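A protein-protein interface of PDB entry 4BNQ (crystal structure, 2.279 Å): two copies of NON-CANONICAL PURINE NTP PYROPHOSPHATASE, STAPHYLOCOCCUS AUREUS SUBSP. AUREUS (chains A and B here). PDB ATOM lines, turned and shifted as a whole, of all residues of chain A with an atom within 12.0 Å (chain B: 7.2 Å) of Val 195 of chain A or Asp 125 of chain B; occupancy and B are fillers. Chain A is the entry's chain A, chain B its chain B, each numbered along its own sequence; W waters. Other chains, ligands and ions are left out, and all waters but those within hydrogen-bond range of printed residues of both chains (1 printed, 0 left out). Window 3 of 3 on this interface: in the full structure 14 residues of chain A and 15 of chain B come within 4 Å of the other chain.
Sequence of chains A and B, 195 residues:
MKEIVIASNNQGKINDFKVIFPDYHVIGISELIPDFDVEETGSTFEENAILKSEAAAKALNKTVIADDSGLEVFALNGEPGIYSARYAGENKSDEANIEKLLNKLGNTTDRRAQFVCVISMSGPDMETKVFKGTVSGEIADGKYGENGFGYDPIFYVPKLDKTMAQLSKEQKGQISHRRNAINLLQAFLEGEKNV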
ATOM      1  N   GLN A 186     -16.854 -12.819 -23.286  1.00  0.00           N
ATOM      2  CA  GLN A 186     -17.527 -11.620 -22.801  1.00  0.00           C
ATOM      3  C   GLN A 186     -18.464 -11.043 -23.841  1.00  0.00           C
ATOM      4  O   GLN A 186     -19.529 -10.526 -23.492  1.00  0.00           O
ATOM      5  CB  GLN A 186     -16.519 -10.575 -22.304  1.00  0.00           C
ATOM      6  CG  GLN A 186     -16.061 -10.864 -20.873  1.00  0.00           C
ATOM      7  CD  GLN A 186     -14.894 -10.012 -20.447  1.00  0.00           C
ATOM      8  OE1 GLN A 186     -14.167  -9.466 -21.284  1.00  0.00           O
ATOM      9  NE2 GLN A 186     -14.706  -9.881 -19.140  1.00  0.00           N
ATOM     10  N   ALA A 187     -18.081 -11.154 -25.113  1.00  0.00           N
ATOM     11  CA  ALA A 187     -18.956 -10.714 -26.201  1.00  0.00           C
ATOM     12  C   ALA A 187     -20.200 -11.589 -26.242  1.00  0.00           C
ATOM     13  O   ALA A 187     -21.300 -11.101 -26.474  1.00  0.00           O
ATOM     14  CB  ALA A 187     -18.235 -10.743 -27.547  1.00  0.00           C
ATOM     15  N   PHE A 188     -20.009 -12.886 -26.025  1.00  0.00           N
ATOM     16  CA  PHE A 188     -21.114 -13.827 -25.955  1.00  0.00           C
ATOM     17  C   PHE A 188     -22.085 -13.445 -24.826  1.00  0.00           C
ATOM     18  O   PHE A 188     -23.298 -13.408 -25.021  1.00  0.00           O
ATOM     19  CB  PHE A 188     -20.568 -15.243 -25.748  1.00  0.00           C
ATOM     20  CG  PHE A 188     -21.632 -16.302 -25.675  1.00  0.00           C
ATOM     21  CD1 PHE A 188     -22.222 -16.642 -24.456  1.00  0.00           C
ATOM     22  CD2 PHE A 188     -22.043 -16.966 -26.820  1.00  0.00           C
ATOM     23  CE1 PHE A 188     -23.211 -17.623 -24.388  1.00  0.00           C
ATOM     24  CE2 PHE A 188     -23.027 -17.948 -26.759  1.00  0.00           C
ATOM     25  CZ  PHE A 188     -23.611 -18.279 -25.538  1.00  0.00           C
ATOM     26  N   LEU A 189     -21.534 -13.168 -23.649  1.00  0.00           N
ATOM     27  CA  LEU A 189     -22.322 -12.746 -22.495  1.00  0.00           C
ATOM     28  C   LEU A 189     -23.077 -11.436 -22.760  1.00  0.00           C
ATOM     29  O   LEU A 189     -24.223 -11.266 -22.332  1.00  0.00           O
ATOM     30  CB  LEU A 189     -21.420 -12.567 -21.271  1.00  0.00           C
ATOM     31  CG  LEU A 189     -20.624 -13.795 -20.809  1.00  0.00           C
ATOM     32  CD1 LEU A 189     -19.680 -13.430 -19.654  1.00  0.00           C
ATOM     33  CD2 LEU A 189     -21.565 -14.893 -20.391  1.00  0.00           C
ATOM     34  N   GLU A 190     -22.426 -10.510 -23.457  1.00  0.00           N
ATOM     35  CA  GLU A 190     -23.049  -9.238 -23.789  1.00  0.00           C
ATOM     36  C   GLU A 190     -24.191  -9.463 -24.779  1.00  0.00           C
ATOM     37  O   GLU A 190     -25.219  -8.790 -24.708  1.00  0.00           O
ATOM     38  CB  GLU A 190     -22.016  -8.246 -24.350  1.00  0.00           C
ATOM     39  CG  GLU A 190     -21.155  -7.563 -23.288  1.00  0.00           C
ATOM     40  CD  GLU A 190     -21.925  -6.536 -22.455  1.00  0.00           C
ATOM     41  OE1 GLU A 190     -22.510  -5.599 -23.048  1.00  0.00           O
ATOM     42  OE2 GLU A 190     -21.937  -6.650 -21.204  1.00  0.00           O
ATOM     43  N   GLY A 191     -24.008 -10.416 -25.688  1.00  0.00           N
ATOM     44  CA  GLY A 191     -25.059 -10.821 -26.605  1.00  0.00           C
ATOM     45  C   GLY A 191     -26.305 -11.365 -25.912  1.00  0.00           C
ATOM     46  O   GLY A 191     -27.419 -11.151 -26.403  1.00  0.00           O
ATOM     47  N   GLU A 192     -26.135 -12.060 -24.782  1.00  0.00           N
ATOM     48  CA  GLU A 192     -27.295 -12.637 -24.096  1.00  0.00           C
ATOM     49  C   GLU A 192     -27.990 -11.653 -23.159  1.00  0.00           C
ATOM     50  O   GLU A 192     -28.984 -11.980 -22.518  1.00  0.00           O
ATOM     51  CB  GLU A 192     -26.997 -13.997 -23.424  1.00  0.00           C
ATOM     52  CG  GLU A 192     -26.116 -14.014 -22.180  1.00  0.00           C
ATOM     53  CD  GLU A 192     -25.734 -15.450 -21.765  1.00  0.00           C
ATOM     54  OE1 GLU A 192     -26.001 -16.402 -22.541  1.00  0.00           O
ATOM     55  OE2 GLU A 192     -25.167 -15.637 -20.662  1.00  0.00           O
ATOM     56  N   LYS A 193     -27.479 -10.435 -23.099  1.00  0.00           N
ATOM     57  CA  LYS A 193     -28.212  -9.379 -22.435  1.00  0.00           C
ATOM     58  C   LYS A 193     -29.140  -8.699 -23.445  1.00  0.00           C
ATOM     59  O   LYS A 193     -29.194  -7.477 -23.523  1.00  0.00           O
ATOM     60  CB  LYS A 193     -27.257  -8.381 -21.801  1.00  0.00           C
ATOM     61  CG  LYS A 193     -26.351  -8.983 -20.744  1.00  0.00           C
ATOM     62  CD  LYS A 193     -25.530  -7.868 -20.131  1.00  0.00           C
ATOM     63  CE  LYS A 193     -24.560  -8.358 -19.086  1.00  0.00           C
ATOM     64  NZ  LYS A 193     -23.648  -7.229 -18.719  1.00  0.00           N
ATOM     65  N   ASN A 194     -29.855  -9.520 -24.217  1.00  0.00           N
ATOM     66  CA  ASN A 194     -30.869  -9.060 -25.164  1.00  0.00           C
ATOM     67  C   ASN A 194     -30.354  -8.051 -26.174  1.00  0.00           C
ATOM     68  O   ASN A 194     -30.965  -6.998 -26.353  1.00  0.00           O
ATOM     69  CB  ASN A 194     -32.074  -8.474 -24.424  1.00  0.00           C
ATOM     70  CG  ASN A 194     -32.759  -9.487 -23.541  1.00  0.00           C
ATOM     71  OD1 ASN A 194     -33.390 -10.425 -24.030  1.00  0.00           O
ATOM     72  ND2 ASN A 194     -32.650  -9.302 -22.230  1.00  0.00           N
ATOM     73  N   VAL A 195     -29.234  -8.380 -26.820  1.00  0.00           N
ATOM     74  CA  VAL A 195     -28.609  -7.531 -27.846  1.00  0.00           C
ATOM     75  C   VAL A 195     -28.194  -6.159 -27.316  1.00  0.00           C
ATOM     76  O   VAL A 195     -28.554  -5.743 -26.215  1.00  0.00           O
ATOM     77  CB  VAL A 195     -29.487  -7.395 -29.131  1.00  0.00           C
ATOM     78  CG1 VAL A 195     -30.259  -6.071 -29.154  1.00  0.00           C
ATOM     79  CG2 VAL A 195     -28.640  -7.518 -30.395  1.00  0.00           C
ATOM     80  OXT VAL A 195     -27.458  -5.425 -27.978  1.00  0.00           O
ATOM     81  N   TYR B  24     -31.142 -13.188 -41.251  1.00  0.00           N
ATOM     82  CA  TYR B  24     -31.586 -11.818 -41.466  1.00  0.00           C
ATOM     83  C   TYR B  24     -31.672 -11.430 -42.936  1.00  0.00           C
ATOM     84  O   TYR B  24     -31.084 -12.079 -43.808  1.00  0.00           O
ATOM     85  CB  TYR B  24     -30.633 -10.838 -40.787  1.00  0.00           C
ATOM     86  CG  TYR B  24     -30.578 -10.885 -39.275  1.00  0.00           C
ATOM     87  CD1 TYR B  24     -29.921 -11.912 -38.613  1.00  0.00           C
ATOM     88  CD2 TYR B  24     -31.143  -9.874 -38.509  1.00  0.00           C
ATOM     89  CE1 TYR B  24     -29.847 -11.945 -37.226  1.00  0.00           C
ATOM     90  CE2 TYR B  24     -31.076  -9.900 -37.123  1.00  0.00           C
ATOM     91  CZ  TYR B  24     -30.426 -10.936 -36.489  1.00  0.00           C
ATOM     92  OH  TYR B  24     -30.353 -10.963 -35.114  1.00  0.00           O
ATOM     93  N   ASN B  61     -34.204   4.064 -37.327  1.00  0.00           N
ATOM     94  CA  ASN B  61     -34.838   3.180 -36.345  1.00  0.00           C
ATOM     95  C   ASN B  61     -34.592   1.708 -36.703  1.00  0.00           C
ATOM     96  O   ASN B  61     -35.465   0.872 -36.534  1.00  0.00           O
ATOM     97  CB  ASN B  61     -36.344   3.451 -36.268  1.00  0.00           C
ATOM     98  CG  ASN B  61     -36.945   3.069 -34.940  1.00  0.00           C
ATOM     99  OD1 ASN B  61     -36.289   3.147 -33.894  1.00  0.00           O
ATOM    100  ND2 ASN B  61     -38.214   2.669 -34.967  1.00  0.00           N
ATOM    101  N   THR B  63     -31.343  -1.596 -36.958  1.00  0.00           N
ATOM    102  CA  THR B  63     -30.042  -2.055 -36.488  1.00  0.00           C
ATOM    103  C   THR B  63     -29.038  -1.975 -37.632  1.00  0.00           C
ATOM    104  O   THR B  63     -29.297  -2.461 -38.738  1.00  0.00           O
ATOM    105  CB  THR B  63     -30.120  -3.503 -35.961  1.00  0.00           C
ATOM    106  OG1 THR B  63     -30.890  -3.521 -34.751  1.00  0.00           O
ATOM    107  CG2 THR B  63     -28.734  -4.049 -35.688  1.00  0.00           C
ATOM    108  N   MET B 121     -21.931  -1.714 -33.908  1.00  0.00           N
ATOM    109  CA  MET B 121     -23.321  -2.090 -34.154  1.00  0.00           C
ATOM    110  C   MET B 121     -24.230  -1.210 -33.305  1.00  0.00           C
ATOM    111  O   MET B 121     -24.090  -1.156 -32.083  1.00  0.00           O
ATOM    112  CB  MET B 121     -23.579  -3.571 -33.850  1.00  0.00           C
ATOM    113  CG  MET B 121     -24.956  -4.057 -34.350  1.00  0.00           C
ATOM    114  SD  MET B 121     -25.347  -5.818 -34.197  1.00  0.00           S
ATOM    115  CE  MET B 121     -25.030  -6.009 -32.476  1.00  0.00           C
ATOM    116  N   SER B 122     -25.146  -0.500 -33.952  1.00  0.00           N
ATOM    117  CA  SER B 122     -26.057   0.386 -33.230  1.00  0.00           C
ATOM    118  C   SER B 122     -27.485   0.066 -33.616  1.00  0.00           C
ATOM    119  O   SER B 122     -27.743  -0.449 -34.708  1.00  0.00           O
ATOM    120  CB  SER B 122     -25.770   1.854 -33.551  1.00  0.00           C
ATOM    121  OG  SER B 122     -24.452   2.212 -33.195  1.00  0.00           O
ATOM    122  N   GLY B 123     -28.412   0.378 -32.724  1.00  0.00           N
ATOM    123  CA  GLY B 123     -29.812   0.088 -32.955  1.00  0.00           C
ATOM    124  C   GLY B 123     -30.705   0.699 -31.894  1.00  0.00           C
ATOM    125  O   GLY B 123     -30.219   1.284 -30.920  1.00  0.00           O
ATOM    126  N   PRO B 124     -32.026   0.557 -32.075  1.00  0.00           N
ATOM    127  CA  PRO B 124     -33.017   1.154 -31.166  1.00  0.00           C
ATOM    128  C   PRO B 124     -33.115   0.475 -29.789  1.00  0.00           C
ATOM    129  O   PRO B 124     -33.133   1.173 -28.775  1.00  0.00           O
ATOM    130  CB  PRO B 124     -34.337   1.003 -31.937  1.00  0.00           C
ATOM    131  CG  PRO B 124     -34.106  -0.143 -32.891  1.00  0.00           C
ATOM    132  CD  PRO B 124     -32.645  -0.102 -33.242  1.00  0.00           C
ATOM    133  N   ASP B 125     -33.186  -0.851 -29.746  1.00  0.00           N
ATOM    134  CA  ASP B 125     -33.393  -1.549 -28.469  1.00  0.00           C
ATOM    135  C   ASP B 125     -32.073  -2.026 -27.868  1.00  0.00           C
ATOM    136  O   ASP B 125     -31.958  -3.184 -27.443  1.00  0.00           O
ATOM    137  CB  ASP B 125     -34.323  -2.753 -28.657  1.00  0.00           C
ATOM    138  CG  ASP B 125     -35.470  -2.463 -29.602  1.00  0.00           C
ATOM    139  OD1 ASP B 125     -36.442  -1.808 -29.165  1.00  0.00           O
ATOM    140  OD2 ASP B 125     -35.398  -2.894 -30.777  1.00  0.00           O
ATOM    141  N   MET B 126     -31.096  -1.124 -27.804  1.00  0.00           N
ATOM    142  CA  MET B 126     -29.709  -1.541 -27.659  1.00  0.00           C
ATOM    143  C   MET B 126     -28.748  -0.353 -27.534  1.00  0.00           C
ATOM    144  O   MET B 126     -28.910   0.656 -28.207  1.00  0.00           O
ATOM    145  CB  MET B 126     -29.361  -2.391 -28.883  1.00  0.00           C
ATOM    146  CG  MET B 126     -27.919  -2.512 -29.187  1.00  0.00           C
ATOM    147  SD  MET B 126     -27.640  -3.422 -30.707  1.00  0.00           S
ATOM    148  CE  MET B 126     -25.872  -3.274 -30.670  1.00  0.00           C
ATOM    149  N   GLU B 127     -27.761  -0.459 -26.654  1.00  0.00           N
ATOM    150  CA  GLU B 127     -26.674   0.512 -26.635  1.00  0.00           C
ATOM    151  C   GLU B 127     -25.656   0.106 -27.704  1.00  0.00           C
ATOM    152  O   GLU B 127     -25.506  -1.075 -27.991  1.00  0.00           O
ATOM    153  CB  GLU B 127     -26.012   0.545 -25.257  1.00  0.00           C
ATOM    154  CG  GLU B 127     -26.877   1.158 -24.172  1.00  0.00           C
ATOM    155  CD  GLU B 127     -27.147   2.634 -24.413  1.00  0.00           C
ATOM    156  OE1 GLU B 127     -26.230   3.335 -24.901  1.00  0.00           O
ATOM    157  OE2 GLU B 127     -28.274   3.098 -24.116  1.00  0.00           O
ATOM    158  N   THR B 128     -24.962   1.078 -28.289  1.00  0.00           N
ATOM    159  CA  THR B 128     -24.004   0.798 -29.355  1.00  0.00           C
ATOM    160  C   THR B 128     -22.865  -0.120 -28.887  1.00  0.00           C
ATOM    161  O   THR B 128     -22.275   0.101 -27.826  1.00  0.00           O
ATOM    162  CB  THR B 128     -23.417   2.097 -29.935  1.00  0.00           C
ATOM    163  OG1 THR B 128     -24.417   2.762 -30.711  1.00  0.00           O
ATOM    164  CG2 THR B 128     -22.223   1.790 -30.826  1.00  0.00           C
ATOM    165  N   LYS B 129     -22.568  -1.144 -29.686  1.00  0.00           N
ATOM    166  CA  LYS B 129     -21.526  -2.118 -29.364  1.00  0.00           C
ATOM    167  C   LYS B 129     -20.340  -2.048 -30.309  1.00  0.00           C
ATOM    168  O   LYS B 129     -20.515  -1.866 -31.509  1.00  0.00           O
ATOM    169  CB  LYS B 129     -22.090  -3.535 -29.387  1.00  0.00           C
ATOM    170  CG  LYS B 129     -22.403  -4.074 -28.005  1.00  0.00           C
ATOM    171  CD  LYS B 129     -23.833  -3.780 -27.593  1.00  0.00           C
ATOM    172  CE  LYS B 129     -24.014  -3.980 -26.097  1.00  0.00           C
ATOM    173  NZ  LYS B 129     -23.101  -3.073 -25.347  1.00  0.00           N
ATOM    174  N   PHE B 188     -21.099 -12.397 -30.088  1.00  0.00           N
ATOM    175  CA  PHE B 188     -22.187 -11.580 -29.579  1.00  0.00           C
ATOM    176  C   PHE B 188     -23.510 -12.084 -30.130  1.00  0.00           C
ATOM    177  O   PHE B 188     -24.468 -12.285 -29.384  1.00  0.00           O
ATOM    178  CB  PHE B 188     -21.991 -10.128 -30.008  1.00  0.00           C
ATOM    179  CG  PHE B 188     -23.069  -9.198 -29.523  1.00  0.00           C
ATOM    180  CD1 PHE B 188     -24.215  -8.974 -30.277  1.00  0.00           C
ATOM    181  CD2 PHE B 188     -22.937  -8.542 -28.308  1.00  0.00           C
ATOM    182  CE1 PHE B 188     -25.219  -8.110 -29.817  1.00  0.00           C
ATOM    183  CE2 PHE B 188     -23.933  -7.677 -27.848  1.00  0.00           C
ATOM    184  CZ  PHE B 188     -25.072  -7.461 -28.608  1.00  0.00           C
ATOM    185  N   LEU B 189     -23.561 -12.257 -31.449  1.00  0.00           N
ATOM    186  CA  LEU B 189     -24.771 -12.715 -32.124  1.00  0.00           C
ATOM    187  C   LEU B 189     -25.176 -14.085 -31.617  1.00  0.00           C
ATOM    188  O   LEU B 189     -26.347 -14.326 -31.338  1.00  0.00           O
ATOM    189  CB  LEU B 189     -24.561 -12.763 -33.632  1.00  0.00           C
ATOM    190  CG  LEU B 189     -24.419 -11.413 -34.330  1.00  0.00           C
ATOM    191  CD1 LEU B 189     -24.089 -11.642 -35.802  1.00  0.00           C
ATOM    192  CD2 LEU B 189     -25.691 -10.586 -34.159  1.00  0.00           C
ATOM    193  N   GLY B 191     -24.518 -15.093 -28.836  1.00  0.00           N
ATOM    194  CA  GLY B 191     -24.874 -14.851 -27.453  1.00  0.00           C
ATOM    195  C   GLY B 191     -26.359 -14.650 -27.252  1.00  0.00           C
ATOM    196  O   GLY B 191     -26.900 -15.043 -26.216  1.00  0.00           O
ATOM    197  N   GLU B 192     -27.025 -14.061 -28.245  1.00  0.00           N
ATOM    198  CA  GLU B 192     -28.447 -13.759 -28.115  1.00  0.00           C
ATOM    199  C   GLU B 192     -29.344 -14.923 -28.530  1.00  0.00           C
ATOM    200  O   GLU B 192     -30.421 -14.724 -29.092  1.00  0.00           O
ATOM    201  CB  GLU B 192     -28.820 -12.469 -28.860  1.00  0.00           C
ATOM    202  CG  GLU B 192     -28.636 -12.483 -30.370  1.00  0.00           C
ATOM    203  CD  GLU B 192     -28.332 -11.094 -30.883  1.00  0.00           C
ATOM    204  OE1 GLU B 192     -27.806 -10.304 -30.074  1.00  0.00           O
ATOM    205  OE2 GLU B 192     -28.612 -10.781 -32.065  1.00  0.00           O
HETATM  206  O   HOH W   1     -28.020  -3.364 -24.757  1.00  0.00           O
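NZ of Lys 129 of chain B lies within salt-bridge range of OE1 of Glu 190 of chain A, 3.5 Å away.
The backbone carbonyl oxygen (O) of Gly 191 of chain A sits close to the backbone NH (N) of Glu 192 of chain B (3.5 Å).
The backbone carbonyl oxygen (O) of Gly 191 of chain B sits close to the backbone NH (N) of Glu 192 of chain A (3.4 Å).
The chain-end carboxylate of Val 195 of chain A sits close to the side-chain sulfur of Met 126 of chain B (3.4 Å).
Phe 188 of chain A touches Gly 191 of chain B, and with the chains exchanged Gly 191 of chain A touches Phe 188 of chain B.
Gly 191 of chain A touches its own counterpart, Gly 191 of chain B.
Gly 191 of chain A touches Glu 192 of chain B, and with the chains exchanged Glu 192 of chain A touches Gly 191 of chain B.
Positions printed for both chains: 188, 189, 191 and 192.
Of the 13 pairs that touch across the chains among the printed residues, 5 have their exchanged pair printed and touching as well.
Water W1 bridges O of Val 195 of chain A (2.8 Å) and N of Glu 127 of chain B (3.5 Å).
Of the 16 printed residues of chain B, 6 touch a printed residue of chain A.
Hydrophobic or aromatic side chains of chain B that line the printed part of chain A: Met 126 and Phe 188.
Of the 10 printed residues of chain A, 6 touch a printed residue of chain B.
Printed residues of chain A that touch a printed residue of chain B: Ala 187, Phe 188, Glu 190, Gly 191, Glu 192 and Val 195.
Hydrophobic or aromatic side chains of chain A that line the printed part of chain B: Phe 188 and Val 195.
Along chain A the printed residues that touch a printed residue of chain B span positions 187 to 195.
Among the printed residues, 13 pairs touch across the chains.
Of the printed residues of chain B, Val 195 of chain A touches Asp 125, Met 126, Lys 129, Phe 188 and Glu 192.
Gly 123 of chain B touches none of the printed residues of chain A.
No residue of chain A comes within 4 Å of Pro 124 of chain B.
Of chain A, only Val 195 comes within 4 Å of Met 126 of chain B.
Glu 192 of chain B touches just these residues of chain A: Gly 191 and Val 195.
Of the printed residues of chain A, Phe 188 of chain B touches Ala 187 (3.3 Å), Glu 190 (3.6 Å), Gly 191 (3.2 Å) and Val 195 (3.2 Å).
Of the printed residues of chain B, Phe 188 of chain A touches Gly 191 (3.2 Å).
Of the printed residues of chain B, Glu 192 of chain A touches Gly 191 (3.0 Å).
Of the printed residues of chain B, Ala 187 of chain A touches Phe 188 (3.3 Å).
The nearest residue of chain A that does not touch Asp 125 of chain B is Asn 194 of chain A (4.1 Å).
Among the printed residues, pairs that only touch across the chains: Val 195 of chain A with Glu 192 of chain B, Gly 191 of chain A with Phe 188 of chain B, Val 195 of chain A with Phe 188 of chain B, Phe 188 of chain A with Gly 191 of chain B, Ala 187 of chain A with Phe 188 of chain B, Gly 191 of chain A with Gly 191 of chain B, Glu 190 of chain A with Phe 188 of chain B, Val 195 of chain A with Asp 125 of chain B and Val 195 of chain A with Lys 129 of chain B.
The side-chain carboxylate (OE2) of Glu 190 of chain A lies within salt-bridge range of the side-chain amino group (NZ) of Lys 193 of chain A.
N of Met 121 of chain B is in hydrogen-bond range of O of Lys 129 of chain B, 2.8 Å away.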
